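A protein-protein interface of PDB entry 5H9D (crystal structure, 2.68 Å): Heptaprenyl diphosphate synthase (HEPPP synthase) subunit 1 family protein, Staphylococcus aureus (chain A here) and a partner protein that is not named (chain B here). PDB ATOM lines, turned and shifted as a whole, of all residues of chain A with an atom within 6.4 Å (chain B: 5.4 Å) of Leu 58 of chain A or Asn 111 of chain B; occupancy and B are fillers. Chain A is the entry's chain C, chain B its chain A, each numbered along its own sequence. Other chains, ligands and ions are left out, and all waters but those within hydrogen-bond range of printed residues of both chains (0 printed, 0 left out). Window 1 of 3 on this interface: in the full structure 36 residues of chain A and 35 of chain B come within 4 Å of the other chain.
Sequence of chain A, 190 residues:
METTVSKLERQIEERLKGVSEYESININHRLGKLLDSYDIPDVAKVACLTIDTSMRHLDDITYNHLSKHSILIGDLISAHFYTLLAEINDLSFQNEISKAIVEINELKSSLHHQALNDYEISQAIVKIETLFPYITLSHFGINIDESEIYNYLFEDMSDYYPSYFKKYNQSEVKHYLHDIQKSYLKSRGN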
ATOM      1  N   THR A  53       1.054   9.475  23.110  1.00  0.00           N
ATOM      2  CA  THR A  53       2.190   8.553  23.130  1.00  0.00           C
ATOM      3  C   THR A  53       3.528   9.229  23.465  1.00  0.00           C
ATOM      4  O   THR A  53       4.252   8.786  24.371  1.00  0.00           O
ATOM      5  CB  THR A  53       2.328   7.801  21.760  1.00  0.00           C
ATOM      6  OG1 THR A  53       1.116   7.099  21.469  1.00  0.00           O
ATOM      7  CG2 THR A  53       3.454   6.801  21.803  1.00  0.00           C
ATOM      8  N   SER A  54       3.876  10.287  22.744  1.00  0.00           N
ATOM      9  CA  SER A  54       5.139  10.945  23.037  1.00  0.00           C
ATOM     10  C   SER A  54       5.129  11.411  24.488  1.00  0.00           C
ATOM     11  O   SER A  54       6.030  11.063  25.270  1.00  0.00           O
ATOM     12  CB  SER A  54       5.378  12.113  22.084  1.00  0.00           C
ATOM     13  OG  SER A  54       4.252  12.963  22.015  1.00  0.00           O
ATOM     14  N   MET A  55       4.087  12.162  24.843  1.00  0.00           N
ATOM     15  CA  MET A  55       3.905  12.681  26.194  1.00  0.00           C
ATOM     16  C   MET A  55       4.112  11.613  27.290  1.00  0.00           C
ATOM     17  O   MET A  55       4.876  11.814  28.235  1.00  0.00           O
ATOM     18  CB  MET A  55       2.509  13.291  26.308  1.00  0.00           C
ATOM     19  CG  MET A  55       2.257  14.538  25.439  1.00  0.00           C
ATOM     20  SD  MET A  55       3.178  15.922  26.030  1.00  0.00           S
ATOM     21  CE  MET A  55       4.672  15.869  24.971  1.00  0.00           C
ATOM     22  N   ARG A  56       3.450  10.465  27.162  1.00  0.00           N
ATOM     23  CA  ARG A  56       3.618   9.409  28.170  1.00  0.00           C
ATOM     24  C   ARG A  56       5.017   8.773  28.105  1.00  0.00           C
ATOM     25  O   ARG A  56       5.518   8.247  29.113  1.00  0.00           O
ATOM     26  CB  ARG A  56       2.542   8.335  28.011  1.00  0.00           C
ATOM     27  CG  ARG A  56       2.689   7.204  29.015  1.00  0.00           C
ATOM     28  CD  ARG A  56       1.531   6.207  28.986  1.00  0.00           C
ATOM     29  NE  ARG A  56       0.231   6.872  29.063  1.00  0.00           N
ATOM     30  CZ  ARG A  56      -0.498   7.195  28.000  1.00  0.00           C
ATOM     31  NH1 ARG A  56      -0.049   6.898  26.783  1.00  0.00           N
ATOM     32  NH2 ARG A  56      -1.661   7.828  28.153  1.00  0.00           N
ATOM     33  N   HIS A  57       5.645   8.836  26.919  1.00  0.00           N
ATOM     34  CA  HIS A  57       6.980   8.284  26.733  1.00  0.00           C
ATOM     35  C   HIS A  57       8.001   9.141  27.436  1.00  0.00           C
ATOM     36  O   HIS A  57       8.860   8.630  28.134  1.00  0.00           O
ATOM     37  CB  HIS A  57       7.338   8.178  25.260  1.00  0.00           C
ATOM     38  CG  HIS A  57       8.558   7.343  24.999  1.00  0.00           C
ATOM     39  ND1 HIS A  57       8.735   6.097  25.560  1.00  0.00           N
ATOM     40  CD2 HIS A  57       9.639   7.556  24.214  1.00  0.00           C
ATOM     41  CE1 HIS A  57       9.870   5.575  25.133  1.00  0.00           C
ATOM     42  NE2 HIS A  57      10.438   6.440  24.312  1.00  0.00           N
ATOM     43  N   LEU A  58       7.891  10.453  27.270  1.00  0.00           N
ATOM     44  CA  LEU A  58       8.818  11.378  27.922  1.00  0.00           C
ATOM     45  C   LEU A  58       8.575  11.352  29.424  1.00  0.00           C
ATOM     46  O   LEU A  58       9.492  11.566  30.219  1.00  0.00           O
ATOM     47  CB  LEU A  58       8.647  12.811  27.360  1.00  0.00           C
ATOM     48  CG  LEU A  58       8.903  13.020  25.850  1.00  0.00           C
ATOM     49  CD1 LEU A  58       8.226  14.252  25.378  1.00  0.00           C
ATOM     50  CD2 LEU A  58      10.379  13.086  25.546  1.00  0.00           C
ATOM     51  N   ASP A  59       7.338  11.091  29.822  1.00  0.00           N
ATOM     52  CA  ASP A  59       7.046  11.022  31.244  1.00  0.00           C
ATOM     53  C   ASP A  59       7.874   9.912  31.834  1.00  0.00           C
ATOM     54  O   ASP A  59       8.631  10.110  32.783  1.00  0.00           O
ATOM     55  CB  ASP A  59       5.584  10.694  31.487  1.00  0.00           C
ATOM     56  CG  ASP A  59       4.737  11.923  31.663  1.00  0.00           C
ATOM     57  OD1 ASP A  59       5.258  12.898  32.254  1.00  0.00           O
ATOM     58  OD2 ASP A  59       3.560  11.904  31.230  1.00  0.00           O
ATOM     59  N   ASP A  60       7.720   8.742  31.225  1.00  0.00           N
ATOM     60  CA  ASP A  60       8.392   7.510  31.620  1.00  0.00           C
ATOM     61  C   ASP A  60       9.902   7.528  31.690  1.00  0.00           C
ATOM     62  O   ASP A  60      10.483   6.840  32.515  1.00  0.00           O
ATOM     63  CB  ASP A  60       7.959   6.371  30.697  1.00  0.00           C
ATOM     64  CG  ASP A  60       6.492   6.029  30.861  1.00  0.00           C
ATOM     65  OD1 ASP A  60       5.955   6.265  31.975  1.00  0.00           O
ATOM     66  OD2 ASP A  60       5.877   5.520  29.896  1.00  0.00           O
ATOM     67  N   ILE A  61      10.541   8.288  30.812  1.00  0.00           N
ATOM     68  CA  ILE A  61      11.987   8.359  30.796  1.00  0.00           C
ATOM     69  C   ILE A  61      12.579   8.651  32.177  1.00  0.00           C
ATOM     70  O   ILE A  61      13.577   8.060  32.566  1.00  0.00           O
ATOM     71  CB  ILE A  61      12.439   9.407  29.743  1.00  0.00           C
ATOM     72  CG1 ILE A  61      12.282   8.792  28.340  1.00  0.00           C
ATOM     73  CG2 ILE A  61      13.870   9.879  30.013  1.00  0.00           C
ATOM     74  CD1 ILE A  61      12.180   9.800  27.225  1.00  0.00           C
ATOM     75  N   THR A  62      11.940   9.527  32.934  1.00  0.00           N
ATOM     76  CA  THR A  62      12.449   9.874  34.248  1.00  0.00           C
ATOM     77  C   THR A  62      12.017   8.889  35.357  1.00  0.00           C
ATOM     78  O   THR A  62      12.634   8.841  36.426  1.00  0.00           O
ATOM     79  CB  THR A  62      12.031  11.331  34.614  1.00  0.00           C
ATOM     80  OG1 THR A  62      12.123  12.168  33.454  1.00  0.00           O
ATOM     81  CG2 THR A  62      12.973  11.911  35.633  1.00  0.00           C
ATOM     82  N   TYR A  63      10.966   8.102  35.102  1.00  0.00           N
ATOM     83  CA  TYR A  63      10.471   7.123  36.086  1.00  0.00           C
ATOM     84  C   TYR A  63      11.012   5.696  35.900  1.00  0.00           C
ATOM     85  O   TYR A  63      11.311   5.008  36.877  1.00  0.00           O
ATOM     86  CB  TYR A  63       8.942   7.056  36.097  1.00  0.00           C
ATOM     87  CG  TYR A  63       8.436   6.287  37.302  1.00  0.00           C
ATOM     88  CD1 TYR A  63       8.863   6.625  38.592  1.00  0.00           C
ATOM     89  CD2 TYR A  63       7.543   5.215  37.164  1.00  0.00           C
ATOM     90  CE1 TYR A  63       8.416   5.911  39.725  1.00  0.00           C
ATOM     91  CE2 TYR A  63       7.088   4.491  38.290  1.00  0.00           C
ATOM     92  CZ  TYR A  63       7.533   4.846  39.566  1.00  0.00           C
ATOM     93  OH  TYR A  63       7.120   4.129  40.674  1.00  0.00           O
ATOM     94  N   SER A  70      16.489   8.484  24.843  1.00  0.00           N
ATOM     95  CA  SER A  70      15.087   8.111  24.730  1.00  0.00           C
ATOM     96  C   SER A  70      14.195   9.348  24.474  1.00  0.00           C
ATOM     97  O   SER A  70      13.116   9.247  23.868  1.00  0.00           O
ATOM     98  CB  SER A  70      14.667   7.410  26.010  1.00  0.00           C
ATOM     99  OG  SER A  70      15.636   6.436  26.338  1.00  0.00           O
ATOM    100  N   ILE A  71      14.666  10.500  24.958  1.00  0.00           N
ATOM    101  CA  ILE A  71      14.001  11.785  24.810  1.00  0.00           C
ATOM    102  C   ILE A  71      13.831  12.124  23.318  1.00  0.00           C
ATOM    103  O   ILE A  71      12.766  12.606  22.903  1.00  0.00           O
ATOM    104  CB  ILE A  71      14.839  12.923  25.494  1.00  0.00           C
ATOM    105  CG1 ILE A  71      15.085  12.593  26.973  1.00  0.00           C
ATOM    106  CG2 ILE A  71      14.123  14.279  25.380  1.00  0.00           C
ATOM    107  CD1 ILE A  71      15.894  13.667  27.726  1.00  0.00           C
ATOM    108  N   LEU A  72      14.869  11.871  22.509  1.00  0.00           N
ATOM    109  CA  LEU A  72      14.792  12.167  21.079  1.00  0.00           C
ATOM    110  C   LEU A  72      13.676  11.393  20.421  1.00  0.00           C
ATOM    111  O   LEU A  72      12.990  11.895  19.534  1.00  0.00           O
ATOM    112  CB  LEU A  72      16.116  11.871  20.398  1.00  0.00           C
ATOM    113  CG  LEU A  72      17.232  12.680  21.070  1.00  0.00           C
ATOM    114  CD1 LEU A  72      18.572  12.201  20.587  1.00  0.00           C
ATOM    115  CD2 LEU A  72      17.039  14.182  20.849  1.00  0.00           C
ATOM    116  N   ILE A  73      13.498  10.159  20.870  1.00  0.00           N
ATOM    117  CA  ILE A  73      12.456   9.286  20.369  1.00  0.00           C
ATOM    118  C   ILE A  73      11.126   9.937  20.694  1.00  0.00           C
ATOM    119  O   ILE A  73      10.281  10.116  19.821  1.00  0.00           O
ATOM    120  CB  ILE A  73      12.497   7.936  21.078  1.00  0.00           C
ATOM    121  CG1 ILE A  73      13.905   7.360  21.010  1.00  0.00           C
ATOM    122  CG2 ILE A  73      11.525   6.991  20.439  1.00  0.00           C
ATOM    123  CD1 ILE A  73      14.321   6.924  19.629  1.00  0.00           C
ATOM    124  N   GLY A  74      10.955  10.302  21.959  1.00  0.00           N
ATOM    125  CA  GLY A  74       9.714  10.914  22.387  1.00  0.00           C
ATOM    126  C   GLY A  74       9.396  12.157  21.610  1.00  0.00           C
ATOM    127  O   GLY A  74       8.234  12.460  21.381  1.00  0.00           O
ATOM    128  N   ASP A  75      10.435  12.881  21.207  1.00  0.00           N
ATOM    129  CA  ASP A  75      10.271  14.106  20.448  1.00  0.00           C
ATOM    130  C   ASP A  75      10.028  13.889  18.954  1.00  0.00           C
ATOM    131  O   ASP A  75       9.413  14.720  18.279  1.00  0.00           O
ATOM    132  CB  ASP A  75      11.481  14.994  20.672  1.00  0.00           C
ATOM    133  CG  ASP A  75      11.446  15.692  22.029  1.00  0.00           C
ATOM    134  OD1 ASP A  75      10.443  16.392  22.327  1.00  0.00           O
ATOM    135  OD2 ASP A  75      12.424  15.545  22.790  1.00  0.00           O
ATOM    136  N   SER A  78       6.627  13.179  18.654  1.00  0.00           N
ATOM    137  CA  SER A  78       5.935  14.430  18.872  1.00  0.00           C
ATOM    138  C   SER A  78       5.921  15.237  17.594  1.00  0.00           C
ATOM    139  O   SER A  78       4.901  15.809  17.235  1.00  0.00           O
ATOM    140  CB  SER A  78       6.611  15.188  20.000  1.00  0.00           C
ATOM    141  OG  SER A  78       5.846  16.318  20.307  1.00  0.00           O
ATOM    142  N   ILE A 101      -2.078  20.729  24.958  1.00  0.00           N
ATOM    143  CA  ILE A 101      -0.742  20.259  25.234  1.00  0.00           C
ATOM    144  C   ILE A 101      -0.010  21.151  26.261  1.00  0.00           C
ATOM    145  O   ILE A 101       0.559  20.636  27.221  1.00  0.00           O
ATOM    146  CB  ILE A 101       0.106  20.132  23.934  1.00  0.00           C
ATOM    147  CG1 ILE A 101      -0.512  19.069  23.010  1.00  0.00           C
ATOM    148  CG2 ILE A 101       1.517  19.643  24.278  1.00  0.00           C
ATOM    149  CD1 ILE A 101       0.151  18.949  21.667  1.00  0.00           C
ATOM    150  N   VAL A 102      -0.020  22.473  26.105  1.00  0.00           N
ATOM    151  CA  VAL A 102       0.692  23.264  27.114  1.00  0.00           C
ATOM    152  C   VAL A 102       0.051  23.073  28.482  1.00  0.00           C
ATOM    153  O   VAL A 102       0.745  23.019  29.478  1.00  0.00           O
ATOM    154  CB  VAL A 102       0.834  24.840  26.765  1.00  0.00           C
ATOM    155  CG1 VAL A 102       0.276  25.166  25.407  1.00  0.00           C
ATOM    156  CG2 VAL A 102       0.219  25.696  27.849  1.00  0.00           C
ATOM    157  N   ASN A 105       1.050  19.764  30.143  1.00  0.00           N
ATOM    158  CA  ASN A 105       2.417  19.980  30.631  1.00  0.00           C
ATOM    159  C   ASN A 105       2.499  20.867  31.857  1.00  0.00           C
ATOM    160  O   ASN A 105       3.283  20.606  32.745  1.00  0.00           O
ATOM    161  CB  ASN A 105       3.280  20.536  29.508  1.00  0.00           C
ATOM    162  CG  ASN A 105       3.595  19.491  28.484  1.00  0.00           C
ATOM    163  OD1 ASN A 105       4.270  18.503  28.759  1.00  0.00           O
ATOM    164  ND2 ASN A 105       3.084  19.683  27.297  1.00  0.00           N
ATOM    165  N   HIS B  81      15.891  20.518  25.897  1.00  0.00           N
ATOM    166  CA  HIS B  81      15.978  19.069  25.850  1.00  0.00           C
ATOM    167  C   HIS B  81      17.403  18.718  25.529  1.00  0.00           C
ATOM    168  O   HIS B  81      17.931  17.723  26.005  1.00  0.00           O
ATOM    169  CB  HIS B  81      15.047  18.462  24.795  1.00  0.00           C
ATOM    170  CG  HIS B  81      13.629  18.267  25.259  1.00  0.00           C
ATOM    171  ND1 HIS B  81      12.709  17.525  24.549  1.00  0.00           N
ATOM    172  CD2 HIS B  81      12.974  18.715  26.357  1.00  0.00           C
ATOM    173  CE1 HIS B  81      11.554  17.524  25.189  1.00  0.00           C
ATOM    174  NE2 HIS B  81      11.688  18.238  26.288  1.00  0.00           N
ATOM    175  N   ALA B 106      12.963  20.059  33.165  1.00  0.00           N
ATOM    176  CA  ALA B 106      13.517  20.390  31.846  1.00  0.00           C
ATOM    177  C   ALA B 106      12.785  19.706  30.708  1.00  0.00           C
ATOM    178  O   ALA B 106      12.575  20.281  29.655  1.00  0.00           O
ATOM    179  CB  ALA B 106      14.999  20.033  31.784  1.00  0.00           C
ATOM    180  N   ILE B 107      12.414  18.464  30.909  1.00  0.00           N
ATOM    181  CA  ILE B 107      11.697  17.762  29.875  1.00  0.00           C
ATOM    182  C   ILE B 107      10.341  18.448  29.695  1.00  0.00           C
ATOM    183  O   ILE B 107       9.907  18.696  28.578  1.00  0.00           O
ATOM    184  CB  ILE B 107      11.543  16.274  30.264  1.00  0.00           C
ATOM    185  CG1 ILE B 107      12.880  15.566  30.062  1.00  0.00           C
ATOM    186  CG2 ILE B 107      10.486  15.592  29.428  1.00  0.00           C
ATOM    187  CD1 ILE B 107      12.860  14.114  30.543  1.00  0.00           C
ATOM    188  N   LEU B 108       9.702  18.780  30.802  1.00  0.00           N
ATOM    189  CA  LEU B 108       8.420  19.419  30.780  1.00  0.00           C
ATOM    190  C   LEU B 108       8.498  20.798  30.163  1.00  0.00           C
ATOM    191  O   LEU B 108       7.597  21.186  29.381  1.00  0.00           O
ATOM    192  CB  LEU B 108       7.836  19.507  32.197  1.00  0.00           C
ATOM    193  CG  LEU B 108       7.247  18.228  32.816  1.00  0.00           C
ATOM    194  CD1 LEU B 108       6.770  18.583  34.203  1.00  0.00           C
ATOM    195  CD2 LEU B 108       6.065  17.671  32.008  1.00  0.00           C
ATOM    196  N   THR B 109       9.570  21.535  30.480  1.00  0.00           N
ATOM    197  CA  THR B 109       9.722  22.885  29.945  1.00  0.00           C
ATOM    198  C   THR B 109       9.847  22.824  28.430  1.00  0.00           C
ATOM    199  O   THR B 109       9.247  23.625  27.716  1.00  0.00           O
ATOM    200  CB  THR B 109      10.933  23.644  30.572  1.00  0.00           C
ATOM    201  OG1 THR B 109      10.842  23.626  32.002  1.00  0.00           O
ATOM    202  CG2 THR B 109      10.878  25.101  30.182  1.00  0.00           C
ATOM    203  N   GLY B 110      10.616  21.848  27.951  1.00  0.00           N
ATOM    204  CA  GLY B 110      10.803  21.662  26.529  1.00  0.00           C
ATOM    205  C   GLY B 110       9.486  21.394  25.823  1.00  0.00           C
ATOM    206  O   GLY B 110       9.254  21.937  24.741  1.00  0.00           O
ATOM    207  N   ASN B 111       8.625  20.560  26.408  1.00  0.00           N
ATOM    208  CA  ASN B 111       7.326  20.263  25.794  1.00  0.00           C
ATOM    209  C   ASN B 111       6.499  21.544  25.750  1.00  0.00           C
ATOM    210  O   ASN B 111       5.822  21.858  24.741  1.00  0.00           O
ATOM    211  CB  ASN B 111       6.543  19.220  26.596  1.00  0.00           C
ATOM    212  CG  ASN B 111       7.262  17.900  26.722  1.00  0.00           C
ATOM    213  OD1 ASN B 111       8.015  17.502  25.840  1.00  0.00           O
ATOM    214  ND2 ASN B 111       7.021  17.207  27.819  1.00  0.00           N
ATOM    215  N   PHE B 112       6.552  22.272  26.864  1.00  0.00           N
ATOM    216  CA  PHE B 112       5.843  23.534  27.006  1.00  0.00           C
ATOM    217  C   PHE B 112       6.223  24.493  25.866  1.00  0.00           C
ATOM    218  O   PHE B 112       5.368  24.959  25.125  1.00  0.00           O
ATOM    219  CB  PHE B 112       6.199  24.100  28.394  1.00  0.00           C
ATOM    220  CG  PHE B 112       5.683  25.479  28.672  1.00  0.00           C
ATOM    221  CD1 PHE B 112       4.333  25.705  28.880  1.00  0.00           C
ATOM    222  CD2 PHE B 112       6.570  26.556  28.782  1.00  0.00           C
ATOM    223  CE1 PHE B 112       3.867  26.983  29.199  1.00  0.00           C
ATOM    224  CE2 PHE B 112       6.114  27.825  29.097  1.00  0.00           C
ATOM    225  CZ  PHE B 112       4.759  28.040  29.307  1.00  0.00           C
ATOM    226  N   LEU B 113       7.520  24.741  25.729  1.00  0.00           N
ATOM    227  CA  LEU B 113       8.081  25.659  24.738  1.00  0.00           C
ATOM    228  C   LEU B 113       7.695  25.279  23.337  1.00  0.00           C
ATOM    229  O   LEU B 113       7.419  26.127  22.490  1.00  0.00           O
ATOM    230  CB  LEU B 113       9.633  25.722  24.875  1.00  0.00           C
ATOM    231  CG  LEU B 113      10.120  26.399  26.171  1.00  0.00           C
ATOM    232  CD1 LEU B 113      11.609  26.408  26.317  1.00  0.00           C
ATOM    233  CD2 LEU B 113       9.622  27.824  26.161  1.00  0.00           C
ATOM    234  N   LEU B 114       7.678  23.980  23.100  1.00  0.00           N
ATOM    235  CA  LEU B 114       7.348  23.442  21.797  1.00  0.00           C
ATOM    236  C   LEU B 114       5.859  23.625  21.504  1.00  0.00           C
ATOM    237  O   LEU B 114       5.495  24.009  20.405  1.00  0.00           O
ATOM    238  CB  LEU B 114       7.691  21.974  21.799  1.00  0.00           C
ATOM    239  CG  LEU B 114       8.113  21.335  20.509  1.00  0.00           C
ATOM    240  CD1 LEU B 114       9.495  21.858  20.154  1.00  0.00           C
ATOM    241  CD2 LEU B 114       8.109  19.805  20.714  1.00  0.00           C
ATOM    242  N   ALA B 115       5.002  23.350  22.489  1.00  0.00           N
ATOM    243  CA  ALA B 115       3.562  23.495  22.282  1.00  0.00           C
ATOM    244  C   ALA B 115       3.207  24.932  21.927  1.00  0.00           C
ATOM    245  O   ALA B 115       2.345  25.173  21.070  1.00  0.00           O
ATOM    246  CB  ALA B 115       2.783  23.058  23.541  1.00  0.00           C
ATOM    247  N   LEU B 116       3.871  25.877  22.603  1.00  0.00           N
ATOM    248  CA  LEU B 116       3.644  27.299  22.370  1.00  0.00           C
ATOM    249  C   LEU B 116       4.060  27.630  20.939  1.00  0.00           C
ATOM    250  O   LEU B 116       3.420  28.437  20.266  1.00  0.00           O
ATOM    251  CB  LEU B 116       4.472  28.142  23.341  1.00  0.00           C
ATOM    252  CG  LEU B 116       4.116  28.210  24.829  1.00  0.00           C
ATOM    253  CD1 LEU B 116       5.211  29.022  25.587  1.00  0.00           C
ATOM    254  CD2 LEU B 116       2.698  28.798  24.980  1.00  0.00           C
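Hydrophobic or aromatic side chains of chain B within 4 Å of the printed part of chain A: His 81, Ile 107, Leu 108 and Ala 115. Of the 21 printed residues of chain A, 8 touch a printed residue of chain B. Among the printed residues, 10 pairs touch across the chains. Among the printed residues, no Asp or Glu carboxylate lies within 4 Å of a Lys or Arg side-chain nitrogen of the other chain.
Among the printed residues, pairs that only touch across the chains: Met 55 of chain A with Asn 111 of chain B (3.7 Å), Leu 58 of chain A with Ile 107 of chain B (3.9 Å), Leu 58 of chain A with Asn 111 of chain B (3.3 Å), Thr 62 of chain A with Ile 107 of chain B (3.6 Å), Ile 71 of chain A with His 81 of chain B (3.6 Å), Ile 101 of chain A with Ala 115 of chain B (3.7 Å), Val 102 of chain A with Ala 115 of chain B (3.8 Å) and Asn 105 of chain A with Leu 108 of chain B (3.8 Å).
Of the printed residues of chain B, Met 55 of chain A touches Asn 111 (3.7 Å). Of chain B, only Ile 107 and Asn 111 come within 4 Å of Leu 58 of chain A. Printed residues of chain B within 4 Å of Thr 62 of chain A: Ile 107. Of the printed residues of chain B, Ile 101 of chain A touches Ala 115. Of the printed residues of chain B, Asn 105 of chain A touches Leu 108 and Asn 111. Printed residues of chain A within 4 Å of Leu 108 of chain B: Asn 105 (3.8 Å). Asn 111 of chain B touches three residues of chain A. The nearest residue of chain B that does not touch Leu 58 of chain A is His 81 of chain B (4.6 Å). The nearest residue of chain A that does not touch Asn 111 of chain B is Asp 75 of chain A (4.4 Å).
O of Ile 107 of chain B lies within hydrogen-bond range of NE2 of His 81 of chain B. ND2 of Asn 111 of chain B lies close to O of Ile 107 of chain B, at 3.3 Å. O of Ile 101 of chain A lies within hydrogen-bond range of ND2 of Asn 105 of chain A.
ND1 of His 81 of chain B lies within hydrogen-bond range of OD2 of Asp 75 of chain A, 2.7 Å away. The side-chain amide nitrogen (ND2) of Asn 111 of chain B sits at hydrogen-bond distance from the side-chain amide oxygen (OD1) of Asn 105 of chain A (3.2 Å).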
